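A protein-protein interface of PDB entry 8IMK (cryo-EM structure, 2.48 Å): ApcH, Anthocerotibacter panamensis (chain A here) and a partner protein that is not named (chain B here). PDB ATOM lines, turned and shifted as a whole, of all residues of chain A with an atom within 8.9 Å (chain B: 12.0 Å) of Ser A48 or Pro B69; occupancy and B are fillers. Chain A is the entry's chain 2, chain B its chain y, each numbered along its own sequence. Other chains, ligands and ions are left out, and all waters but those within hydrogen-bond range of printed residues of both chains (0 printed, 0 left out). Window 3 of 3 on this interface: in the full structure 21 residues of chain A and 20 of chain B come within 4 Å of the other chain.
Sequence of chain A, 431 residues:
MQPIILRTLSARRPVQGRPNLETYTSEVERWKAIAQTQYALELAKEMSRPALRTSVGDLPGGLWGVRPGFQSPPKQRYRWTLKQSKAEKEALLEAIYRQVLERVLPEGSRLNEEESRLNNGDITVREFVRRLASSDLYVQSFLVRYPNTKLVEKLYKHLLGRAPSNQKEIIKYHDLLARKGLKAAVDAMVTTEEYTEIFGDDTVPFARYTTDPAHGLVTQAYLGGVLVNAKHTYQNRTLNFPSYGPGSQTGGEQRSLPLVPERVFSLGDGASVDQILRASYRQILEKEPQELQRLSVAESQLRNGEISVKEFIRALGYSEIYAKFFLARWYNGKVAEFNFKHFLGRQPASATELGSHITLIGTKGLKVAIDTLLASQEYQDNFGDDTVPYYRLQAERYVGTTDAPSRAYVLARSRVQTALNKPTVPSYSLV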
ATOM      1  N   LEU A  41     -11.138 -14.075 -10.187  1.00  0.00           N
ATOM      2  CA  LEU A  41     -10.199 -13.151 -10.816  1.00  0.00           C
ATOM      3  C   LEU A  41      -8.783 -13.708 -10.806  1.00  0.00           C
ATOM      4  O   LEU A  41      -8.069 -13.629 -11.811  1.00  0.00           O
ATOM      5  CB  LEU A  41     -10.243 -11.794 -10.118  1.00  0.00           C
ATOM      6  CG  LEU A  41     -11.339 -10.845 -10.596  1.00  0.00           C
ATOM      7  CD1 LEU A  41     -11.541  -9.723  -9.599  1.00  0.00           C
ATOM      8  CD2 LEU A  41     -11.002 -10.294 -11.967  1.00  0.00           C
ATOM      9  N   GLU A  42      -8.362 -14.289  -9.683  1.00  0.00           N
ATOM     10  CA  GLU A  42      -7.032 -14.883  -9.623  1.00  0.00           C
ATOM     11  C   GLU A  42      -6.921 -16.072 -10.564  1.00  0.00           C
ATOM     12  O   GLU A  42      -5.936 -16.209 -11.306  1.00  0.00           O
ATOM     13  CB  GLU A  42      -6.720 -15.314  -8.193  1.00  0.00           C
ATOM     14  CG  GLU A  42      -7.189 -14.340  -7.135  1.00  0.00           C
ATOM     15  CD  GLU A  42      -6.828 -14.792  -5.737  1.00  0.00           C
ATOM     16  OE1 GLU A  42      -5.619 -14.914  -5.449  1.00  0.00           O
ATOM     17  OE2 GLU A  42      -7.751 -15.036  -4.929  1.00  0.00           O
ATOM     18  N   LEU A  43      -7.928 -16.944 -10.559  1.00  0.00           N
ATOM     19  CA  LEU A  43      -7.824 -18.126 -11.406  1.00  0.00           C
ATOM     20  C   LEU A  43      -7.873 -17.730 -12.882  1.00  0.00           C
ATOM     21  O   LEU A  43      -7.234 -18.361 -13.730  1.00  0.00           O
ATOM     22  CB  LEU A  43      -8.924 -19.124 -11.044  1.00  0.00           C
ATOM     23  CG  LEU A  43      -8.882 -20.525 -11.667  1.00  0.00           C
ATOM     24  CD1 LEU A  43      -9.595 -21.494 -10.734  1.00  0.00           C
ATOM     25  CD2 LEU A  43      -9.420 -20.644 -13.070  1.00  0.00           C
ATOM     26  N   ALA A  44      -8.607 -16.659 -13.200  1.00  0.00           N
ATOM     27  CA  ALA A  44      -8.643 -16.132 -14.557  1.00  0.00           C
ATOM     28  C   ALA A  44      -7.299 -15.553 -14.960  1.00  0.00           C
ATOM     29  O   ALA A  44      -6.854 -15.733 -16.098  1.00  0.00           O
ATOM     30  CB  ALA A  44      -9.732 -15.070 -14.667  1.00  0.00           C
ATOM     31  N   LYS A  45      -6.647 -14.832 -14.045  1.00  0.00           N
ATOM     32  CA  LYS A  45      -5.272 -14.409 -14.274  1.00  0.00           C
ATOM     33  C   LYS A  45      -4.395 -15.601 -14.622  1.00  0.00           C
ATOM     34  O   LYS A  45      -3.506 -15.504 -15.474  1.00  0.00           O
ATOM     35  CB  LYS A  45      -4.740 -13.691 -13.035  1.00  0.00           C
ATOM     36  CG  LYS A  45      -3.300 -13.239 -13.129  1.00  0.00           C
ATOM     37  CD  LYS A  45      -2.961 -12.271 -12.008  1.00  0.00           C
ATOM     38  CE  LYS A  45      -1.459 -12.095 -11.858  1.00  0.00           C
ATOM     39  NZ  LYS A  45      -1.020 -12.202 -10.439  1.00  0.00           N
ATOM     40  N   GLU A  46      -4.631 -16.734 -13.964  1.00  0.00           N
ATOM     41  CA  GLU A  46      -3.899 -17.948 -14.313  1.00  0.00           C
ATOM     42  C   GLU A  46      -4.241 -18.427 -15.722  1.00  0.00           C
ATOM     43  O   GLU A  46      -3.364 -18.899 -16.453  1.00  0.00           O
ATOM     44  CB  GLU A  46      -4.174 -19.046 -13.289  1.00  0.00           C
ATOM     45  CG  GLU A  46      -3.421 -20.336 -13.549  1.00  0.00           C
ATOM     46  CD  GLU A  46      -1.915 -20.179 -13.420  1.00  0.00           C
ATOM     47  OE1 GLU A  46      -1.464 -19.273 -12.687  1.00  0.00           O
ATOM     48  OE2 GLU A  46      -1.180 -20.963 -14.054  1.00  0.00           O
ATOM     49  N   MET A  47      -5.511 -18.324 -16.120  1.00  0.00           N
ATOM     50  CA  MET A  47      -5.922 -18.858 -17.416  1.00  0.00           C
ATOM     51  C   MET A  47      -5.284 -18.108 -18.578  1.00  0.00           C
ATOM     52  O   MET A  47      -5.101 -18.672 -19.663  1.00  0.00           O
ATOM     53  CB  MET A  47      -7.438 -18.816 -17.547  1.00  0.00           C
ATOM     54  CG  MET A  47      -8.159 -19.608 -16.500  1.00  0.00           C
ATOM     55  SD  MET A  47      -9.906 -19.224 -16.487  1.00  0.00           S
ATOM     56  CE  MET A  47     -10.601 -20.861 -16.361  1.00  0.00           C
ATOM     57  N   SER A  48      -4.949 -16.839 -18.385  1.00  0.00           N
ATOM     58  CA  SER A  48      -4.462 -16.032 -19.491  1.00  0.00           C
ATOM     59  C   SER A  48      -2.944 -16.024 -19.608  1.00  0.00           C
ATOM     60  O   SER A  48      -2.394 -15.104 -20.221  1.00  0.00           O
ATOM     61  CB  SER A  48      -4.975 -14.601 -19.358  1.00  0.00           C
ATOM     62  OG  SER A  48      -4.578 -13.822 -20.468  1.00  0.00           O
ATOM     63  N   ARG A  49      -2.260 -17.001 -19.031  1.00  0.00           N
ATOM     64  CA  ARG A  49      -0.818 -17.081 -19.185  1.00  0.00           C
ATOM     65  C   ARG A  49      -0.467 -17.864 -20.451  1.00  0.00           C
ATOM     66  O   ARG A  49      -1.296 -18.619 -20.961  1.00  0.00           O
ATOM     67  CB  ARG A  49      -0.188 -17.731 -17.955  1.00  0.00           C
ATOM     68  CG  ARG A  49      -0.443 -19.212 -17.806  1.00  0.00           C
ATOM     69  CD  ARG A  49       0.576 -19.838 -16.868  1.00  0.00           C
ATOM     70  NE  ARG A  49       0.065 -21.040 -16.218  1.00  0.00           N
ATOM     71  CZ  ARG A  49       0.197 -22.268 -16.706  1.00  0.00           C
ATOM     72  NH1 ARG A  49      -0.298 -23.304 -16.043  1.00  0.00           N
ATOM     73  NH2 ARG A  49       0.822 -22.460 -17.858  1.00  0.00           N
ATOM     74  N   PRO A  50       0.739 -17.694 -20.989  1.00  0.00           N
ATOM     75  CA  PRO A  50       1.088 -18.386 -22.231  1.00  0.00           C
ATOM     76  C   PRO A  50       1.139 -19.896 -22.066  1.00  0.00           C
ATOM     77  O   PRO A  50       1.093 -20.430 -20.958  1.00  0.00           O
ATOM     78  CB  PRO A  50       2.465 -17.814 -22.575  1.00  0.00           C
ATOM     79  CG  PRO A  50       2.489 -16.508 -21.915  1.00  0.00           C
ATOM     80  CD  PRO A  50       1.753 -16.692 -20.635  1.00  0.00           C
ATOM     81  N   ALA A  51       1.272 -20.581 -23.201  1.00  0.00           N
ATOM     82  CA  ALA A  51       0.922 -21.994 -23.269  1.00  0.00           C
ATOM     83  C   ALA A  51       2.036 -22.891 -22.740  1.00  0.00           C
ATOM     84  O   ALA A  51       1.809 -23.708 -21.842  1.00  0.00           O
ATOM     85  CB  ALA A  51       0.566 -22.361 -24.710  1.00  0.00           C
ATOM     86  N   LEU A  52       3.245 -22.765 -23.284  1.00  0.00           N
ATOM     87  CA  LEU A  52       4.278 -23.794 -23.125  1.00  0.00           C
ATOM     88  C   LEU A  52       5.583 -23.159 -22.649  1.00  0.00           C
ATOM     89  O   LEU A  52       6.650 -23.415 -23.206  1.00  0.00           O
ATOM     90  CB  LEU A  52       4.482 -24.559 -24.428  1.00  0.00           C
ATOM     91  CG  LEU A  52       3.389 -25.561 -24.782  1.00  0.00           C
ATOM     92  CD1 LEU A  52       3.411 -25.888 -26.254  1.00  0.00           C
ATOM     93  CD2 LEU A  52       3.557 -26.814 -23.952  1.00  0.00           C
ATOM     94  N   ARG A  53       5.499 -22.332 -21.613  1.00  0.00           N
ATOM     95  CA  ARG A  53       6.647 -21.574 -21.131  1.00  0.00           C
ATOM     96  C   ARG A  53       6.905 -21.896 -19.659  1.00  0.00           C
ATOM     97  O   ARG A  53       7.152 -21.014 -18.840  1.00  0.00           O
ATOM     98  CB  ARG A  53       6.438 -20.077 -21.343  1.00  0.00           C
ATOM     99  CG  ARG A  53       6.242 -19.673 -22.792  1.00  0.00           C
ATOM    100  CD  ARG A  53       7.548 -19.756 -23.565  1.00  0.00           C
ATOM    101  NE  ARG A  53       7.393 -19.375 -24.964  1.00  0.00           N
ATOM    102  CZ  ARG A  53       7.087 -20.221 -25.942  1.00  0.00           C
ATOM    103  NH1 ARG A  53       6.970 -19.780 -27.187  1.00  0.00           N
ATOM    104  NH2 ARG A  53       6.898 -21.506 -25.679  1.00  0.00           N
ATOM    105  N   PHE B  60     -10.311 -30.070 -24.561  1.00  0.00           N
ATOM    106  CA  PHE B  60      -9.592 -28.940 -23.992  1.00  0.00           C
ATOM    107  C   PHE B  60      -9.381 -29.100 -22.497  1.00  0.00           C
ATOM    108  O   PHE B  60      -8.606 -28.350 -21.898  1.00  0.00           O
ATOM    109  CB  PHE B  60     -10.331 -27.652 -24.326  1.00  0.00           C
ATOM    110  CG  PHE B  60     -10.328 -27.341 -25.784  1.00  0.00           C
ATOM    111  CD1 PHE B  60      -9.152 -27.389 -26.499  1.00  0.00           C
ATOM    112  CD2 PHE B  60     -11.492 -27.023 -26.448  1.00  0.00           C
ATOM    113  CE1 PHE B  60      -9.137 -27.116 -27.833  1.00  0.00           C
ATOM    114  CE2 PHE B  60     -11.472 -26.755 -27.792  1.00  0.00           C
ATOM    115  CZ  PHE B  60     -10.294 -26.794 -28.474  1.00  0.00           C
ATOM    116  N   GLN B  63      -6.008 -31.117 -22.834  1.00  0.00           N
ATOM    117  CA  GLN B  63      -4.907 -30.271 -23.289  1.00  0.00           C
ATOM    118  C   GLN B  63      -5.305 -28.811 -23.138  1.00  0.00           C
ATOM    119  O   GLN B  63      -5.760 -28.175 -24.096  1.00  0.00           O
ATOM    120  CB  GLN B  63      -4.524 -30.592 -24.732  1.00  0.00           C
ATOM    121  CG  GLN B  63      -4.171 -32.043 -24.948  1.00  0.00           C
ATOM    122  CD  GLN B  63      -3.297 -32.249 -26.153  1.00  0.00           C
ATOM    123  OE1 GLN B  63      -3.424 -31.546 -27.147  1.00  0.00           O
ATOM    124  NE2 GLN B  63      -2.395 -33.214 -26.072  1.00  0.00           N
ATOM    125  N   PRO B  64      -5.151 -28.249 -21.941  1.00  0.00           N
ATOM    126  CA  PRO B  64      -5.531 -26.843 -21.737  1.00  0.00           C
ATOM    127  C   PRO B  64      -4.630 -25.858 -22.453  1.00  0.00           C
ATOM    128  O   PRO B  64      -5.030 -24.704 -22.637  1.00  0.00           O
ATOM    129  CB  PRO B  64      -5.434 -26.677 -20.214  1.00  0.00           C
ATOM    130  CG  PRO B  64      -5.362 -28.064 -19.670  1.00  0.00           C
ATOM    131  CD  PRO B  64      -4.653 -28.857 -20.702  1.00  0.00           C
ATOM    132  N   ASP B  65      -3.432 -26.273 -22.867  1.00  0.00           N
ATOM    133  CA  ASP B  65      -2.483 -25.336 -23.455  1.00  0.00           C
ATOM    134  C   ASP B  65      -2.931 -24.875 -24.833  1.00  0.00           C
ATOM    135  O   ASP B  65      -2.443 -23.861 -25.342  1.00  0.00           O
ATOM    136  CB  ASP B  65      -1.098 -25.971 -23.528  1.00  0.00           C
ATOM    137  CG  ASP B  65      -0.477 -26.167 -22.165  1.00  0.00           C
ATOM    138  OD1 ASP B  65      -0.787 -25.378 -21.250  1.00  0.00           O
ATOM    139  OD2 ASP B  65       0.326 -27.108 -22.004  1.00  0.00           O
ATOM    140  N   LEU B  66      -3.855 -25.605 -25.457  1.00  0.00           N
ATOM    141  CA  LEU B  66      -4.370 -25.186 -26.753  1.00  0.00           C
ATOM    142  C   LEU B  66      -5.186 -23.906 -26.637  1.00  0.00           C
ATOM    143  O   LEU B  66      -5.227 -23.102 -27.570  1.00  0.00           O
ATOM    144  CB  LEU B  66      -5.207 -26.306 -27.372  1.00  0.00           C
ATOM    145  CG  LEU B  66      -4.531 -27.656 -27.626  1.00  0.00           C
ATOM    146  CD1 LEU B  66      -5.580 -28.719 -27.854  1.00  0.00           C
ATOM    147  CD2 LEU B  66      -3.585 -27.588 -28.803  1.00  0.00           C
ATOM    148  N   LEU B  67      -5.839 -23.697 -25.495  1.00  0.00           N
ATOM    149  CA  LEU B  67      -6.677 -22.516 -25.324  1.00  0.00           C
ATOM    150  C   LEU B  67      -5.866 -21.318 -24.852  1.00  0.00           C
ATOM    151  O   LEU B  67      -6.284 -20.171 -25.028  1.00  0.00           O
ATOM    152  CB  LEU B  67      -7.800 -22.819 -24.337  1.00  0.00           C
ATOM    153  CG  LEU B  67      -8.827 -23.849 -24.785  1.00  0.00           C
ATOM    154  CD1 LEU B  67      -9.884 -24.030 -23.725  1.00  0.00           C
ATOM    155  CD2 LEU B  67      -9.435 -23.437 -26.105  1.00  0.00           C
ATOM    156  N   ARG B  68      -4.716 -21.564 -24.237  1.00  0.00           N
ATOM    157  CA  ARG B  68      -3.919 -20.487 -23.682  1.00  0.00           C
ATOM    158  C   ARG B  68      -3.259 -19.686 -24.803  1.00  0.00           C
ATOM    159  O   ARG B  68      -3.077 -20.194 -25.911  1.00  0.00           O
ATOM    160  CB  ARG B  68      -2.875 -21.050 -22.726  1.00  0.00           C
ATOM    161  CG  ARG B  68      -3.494 -21.748 -21.541  1.00  0.00           C
ATOM    162  CD  ARG B  68      -2.838 -21.374 -20.237  1.00  0.00           C
ATOM    163  NE  ARG B  68      -3.298 -22.224 -19.149  1.00  0.00           N
ATOM    164  CZ  ARG B  68      -2.843 -23.447 -18.903  1.00  0.00           C
ATOM    165  NH1 ARG B  68      -3.332 -24.143 -17.887  1.00  0.00           N
ATOM    166  NH2 ARG B  68      -1.899 -23.975 -19.664  1.00  0.00           N
ATOM    167  N   PRO B  69      -2.916 -18.426 -24.547  1.00  0.00           N
ATOM    168  CA  PRO B  69      -2.269 -17.607 -25.579  1.00  0.00           C
ATOM    169  C   PRO B  69      -1.021 -18.274 -26.135  1.00  0.00           C
ATOM    170  O   PRO B  69      -0.201 -18.815 -25.395  1.00  0.00           O
ATOM    171  CB  PRO B  69      -1.936 -16.313 -24.834  1.00  0.00           C
ATOM    172  CG  PRO B  69      -2.960 -16.230 -23.771  1.00  0.00           C
ATOM    173  CD  PRO B  69      -3.327 -17.625 -23.384  1.00  0.00           C
ATOM    174  N   GLY B  70      -0.883 -18.231 -27.456  1.00  0.00           N
ATOM    175  CA  GLY B  70       0.134 -18.989 -28.142  1.00  0.00           C
ATOM    176  C   GLY B  70      -0.268 -20.397 -28.522  1.00  0.00           C
ATOM    177  O   GLY B  70       0.439 -21.028 -29.313  1.00  0.00           O
ATOM    178  N   GLY B  71      -1.375 -20.910 -27.981  1.00  0.00           N
ATOM    179  CA  GLY B  71      -1.875 -22.199 -28.398  1.00  0.00           C
ATOM    180  C   GLY B  71      -2.575 -22.136 -29.736  1.00  0.00           C
ATOM    181  O   GLY B  71      -3.013 -21.083 -30.185  1.00  0.00           O
ATOM    182  N   ASN B  72      -2.693 -23.294 -30.387  1.00  0.00           N
ATOM    183  CA  ASN B  72      -3.260 -23.297 -31.731  1.00  0.00           C
ATOM    184  C   ASN B  72      -4.770 -23.114 -31.705  1.00  0.00           C
ATOM    185  O   ASN B  72      -5.381 -22.879 -32.750  1.00  0.00           O
ATOM    186  CB  ASN B  72      -2.887 -24.581 -32.474  1.00  0.00           C
ATOM    187  CG  ASN B  72      -3.251 -24.522 -33.957  1.00  0.00           C
ATOM    188  OD1 ASN B  72      -4.341 -24.926 -34.359  1.00  0.00           O
ATOM    189  ND2 ASN B  72      -2.346 -23.990 -34.767  1.00  0.00           N
ATOM    190  N   ALA B  73      -5.389 -23.209 -30.538  1.00  0.00           N
ATOM    191  CA  ALA B  73      -6.803 -22.896 -30.412  1.00  0.00           C
ATOM    192  C   ALA B  73      -7.059 -21.622 -29.619  1.00  0.00           C
ATOM    193  O   ALA B  73      -8.158 -21.458 -29.085  1.00  0.00           O
ATOM    194  CB  ALA B  73      -7.548 -24.065 -29.770  1.00  0.00           C
ATOM    195  N   TYR B  74      -6.078 -20.731 -29.516  1.00  0.00           N
ATOM    196  CA  TYR B  74      -6.298 -19.450 -28.863  1.00  0.00           C
ATOM    197  C   TYR B  74      -6.567 -18.360 -29.887  1.00  0.00           C
ATOM    198  O   TYR B  74      -5.651 -17.866 -30.544  1.00  0.00           O
ATOM    199  CB  TYR B  74      -5.096 -19.056 -28.011  1.00  0.00           C
ATOM    200  CG  TYR B  74      -5.072 -17.587 -27.621  1.00  0.00           C
ATOM    201  CD1 TYR B  74      -5.865 -17.107 -26.589  1.00  0.00           C
ATOM    202  CD2 TYR B  74      -4.249 -16.687 -28.285  1.00  0.00           C
ATOM    203  CE1 TYR B  74      -5.842 -15.783 -26.235  1.00  0.00           C
ATOM    204  CE2 TYR B  74      -4.227 -15.363 -27.942  1.00  0.00           C
ATOM    205  CZ  TYR B  74      -5.019 -14.915 -26.916  1.00  0.00           C
ATOM    206  OH  TYR B  74      -4.986 -13.590 -26.572  1.00  0.00           O
ATOM    207  N   THR B  75      -7.848 -18.111 -30.106  1.00  0.00           N
ATOM    208  CA  THR B  75      -8.527 -16.888 -30.521  1.00  0.00           C
ATOM    209  C   THR B  75      -9.981 -17.312 -30.610  1.00  0.00           C
ATOM    210  O   THR B  75     -10.273 -18.505 -30.525  1.00  0.00           O
ATOM    211  CB  THR B  75      -8.045 -16.262 -31.851  1.00  0.00           C
ATOM    212  OG1 THR B  75      -8.121 -17.200 -32.933  1.00  0.00           O
ATOM    213  CG2 THR B  75      -6.704 -15.528 -31.766  1.00  0.00           C
ATOM    214  N   SER B  76     -10.904 -16.371 -30.760  1.00  0.00           N
ATOM    215  CA  SER B  76     -12.269 -16.777 -31.053  1.00  0.00           C
ATOM    216  C   SER B  76     -12.324 -17.498 -32.391  1.00  0.00           C
ATOM    217  O   SER B  76     -13.042 -18.490 -32.547  1.00  0.00           O
ATOM    218  CB  SER B  76     -13.197 -15.569 -31.050  1.00  0.00           C
ATOM    219  OG  SER B  76     -13.113 -14.869 -32.274  1.00  0.00           O
ATOM    220  N   ARG B  78      -9.906 -19.248 -33.991  1.00  0.00           N
ATOM    221  CA  ARG B  78      -9.302 -20.571 -34.031  1.00  0.00           C
ATOM    222  C   ARG B  78     -10.071 -21.568 -33.175  1.00  0.00           C
ATOM    223  O   ARG B  78     -10.199 -22.738 -33.549  1.00  0.00           O
ATOM    224  CB  ARG B  78      -7.835 -20.486 -33.631  1.00  0.00           C
ATOM    225  CG  ARG B  78      -6.984 -19.936 -34.757  1.00  0.00           C
ATOM    226  CD  ARG B  78      -5.574 -20.443 -34.698  1.00  0.00           C
ATOM    227  NE  ARG B  78      -4.957 -20.186 -33.408  1.00  0.00           N
ATOM    228  CZ  ARG B  78      -4.213 -19.121 -33.141  1.00  0.00           C
ATOM    229  NH1 ARG B  78      -4.002 -18.210 -34.075  1.00  0.00           N
ATOM    230  NH2 ARG B  78      -3.688 -18.968 -31.937  1.00  0.00           N
ATOM    231  N   TYR B  79     -10.632 -21.129 -32.048  1.00  0.00           N
ATOM    232  CA  TYR B  79     -11.545 -22.008 -31.327  1.00  0.00           C
ATOM    233  C   TYR B  79     -12.739 -22.373 -32.200  1.00  0.00           C
ATOM    234  O   TYR B  79     -13.176 -23.532 -32.221  1.00  0.00           O
ATOM    235  CB  TYR B  79     -12.017 -21.362 -30.021  1.00  0.00           C
ATOM    236  CG  TYR B  79     -12.971 -22.254 -29.265  1.00  0.00           C
ATOM    237  CD1 TYR B  79     -14.330 -22.252 -29.548  1.00  0.00           C
ATOM    238  CD2 TYR B  79     -12.509 -23.133 -28.309  1.00  0.00           C
ATOM    239  CE1 TYR B  79     -15.192 -23.082 -28.896  1.00  0.00           C
ATOM    240  CE2 TYR B  79     -13.366 -23.966 -27.651  1.00  0.00           C
ATOM    241  CZ  TYR B  79     -14.707 -23.936 -27.944  1.00  0.00           C
ATOM    242  OH  TYR B  79     -15.570 -24.767 -27.280  1.00  0.00           O
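Ser A48 touches just one residue of chain B: Pro B69. Pro B69 touches just these residues of chain A: Ser A48 (3.8 Å), Arg A49 (3.3 Å), Pro A50 (3.4 Å) and Ala A51 (3.2 Å). No residue of chain B comes within 4 Å of Ala A44. Of chain B, only Arg B68 (3.6 Å) comes within 4 Å of Met A47. Pro A50 touches one residue of chain B. Ala A51 touches just these residues of chain B: Asp B65, Arg B68 and Pro B69. Printed residues of chain B within 4 Å of Arg A49: Arg B68 and Pro B69. Printed residues of chain A within 4 Å of Asp B65: Ala A51 and Leu A52. Leu B66 touches none of the printed residues of chain A. The nearest residue of chain B that does not touch Ser A48 is Arg B68 (5.3 Å).
Among the printed residues, merely in contact across the chains: Arg A49 with Arg B68 (3.2 Å), Arg A49 with Pro B69 (3.3 Å), Pro A50 with Pro B69 (3.4 Å), Met A47 with Arg B68 (3.6 Å), Ser A48 with Pro B69 (3.8 Å), Leu A52 with Asp B65 (3.8 Å) and Ala A51 with Arg B68 (3.95 Å).
The side-chain carboxylate of Glu A46 is in salt-bridge range of the guanidinium group of Arg A49, at 2.5 Å.
The backbone carbonyl oxygen of Pro B69 lies within hydrogen-bond range of the backbone NH of Ala A51 (3.2 Å). O of Ala A51 lies close to OD1 of Asp B65.
Of the 17 printed residues of chain B, 3 touch a printed residue of chain A. Printed residues of chain B that touch a printed residue of chain A: Asp B65, Arg B68 and Pro B69. Hydrophobic or aromatic side chains of chain B within 4 Å of the printed part of chain A: Pro B69. Of the 13 printed residues of chain A, 6 touch a printed residue of chain B. Hydrophobic or aromatic side chains of chain A within 4 Å of the printed part of chain B: Ala A51 and Leu A52. Among the printed residues, no Asp or Glu carboxylate lies within 4 Å of a Lys or Arg side-chain nitrogen of the other chain.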
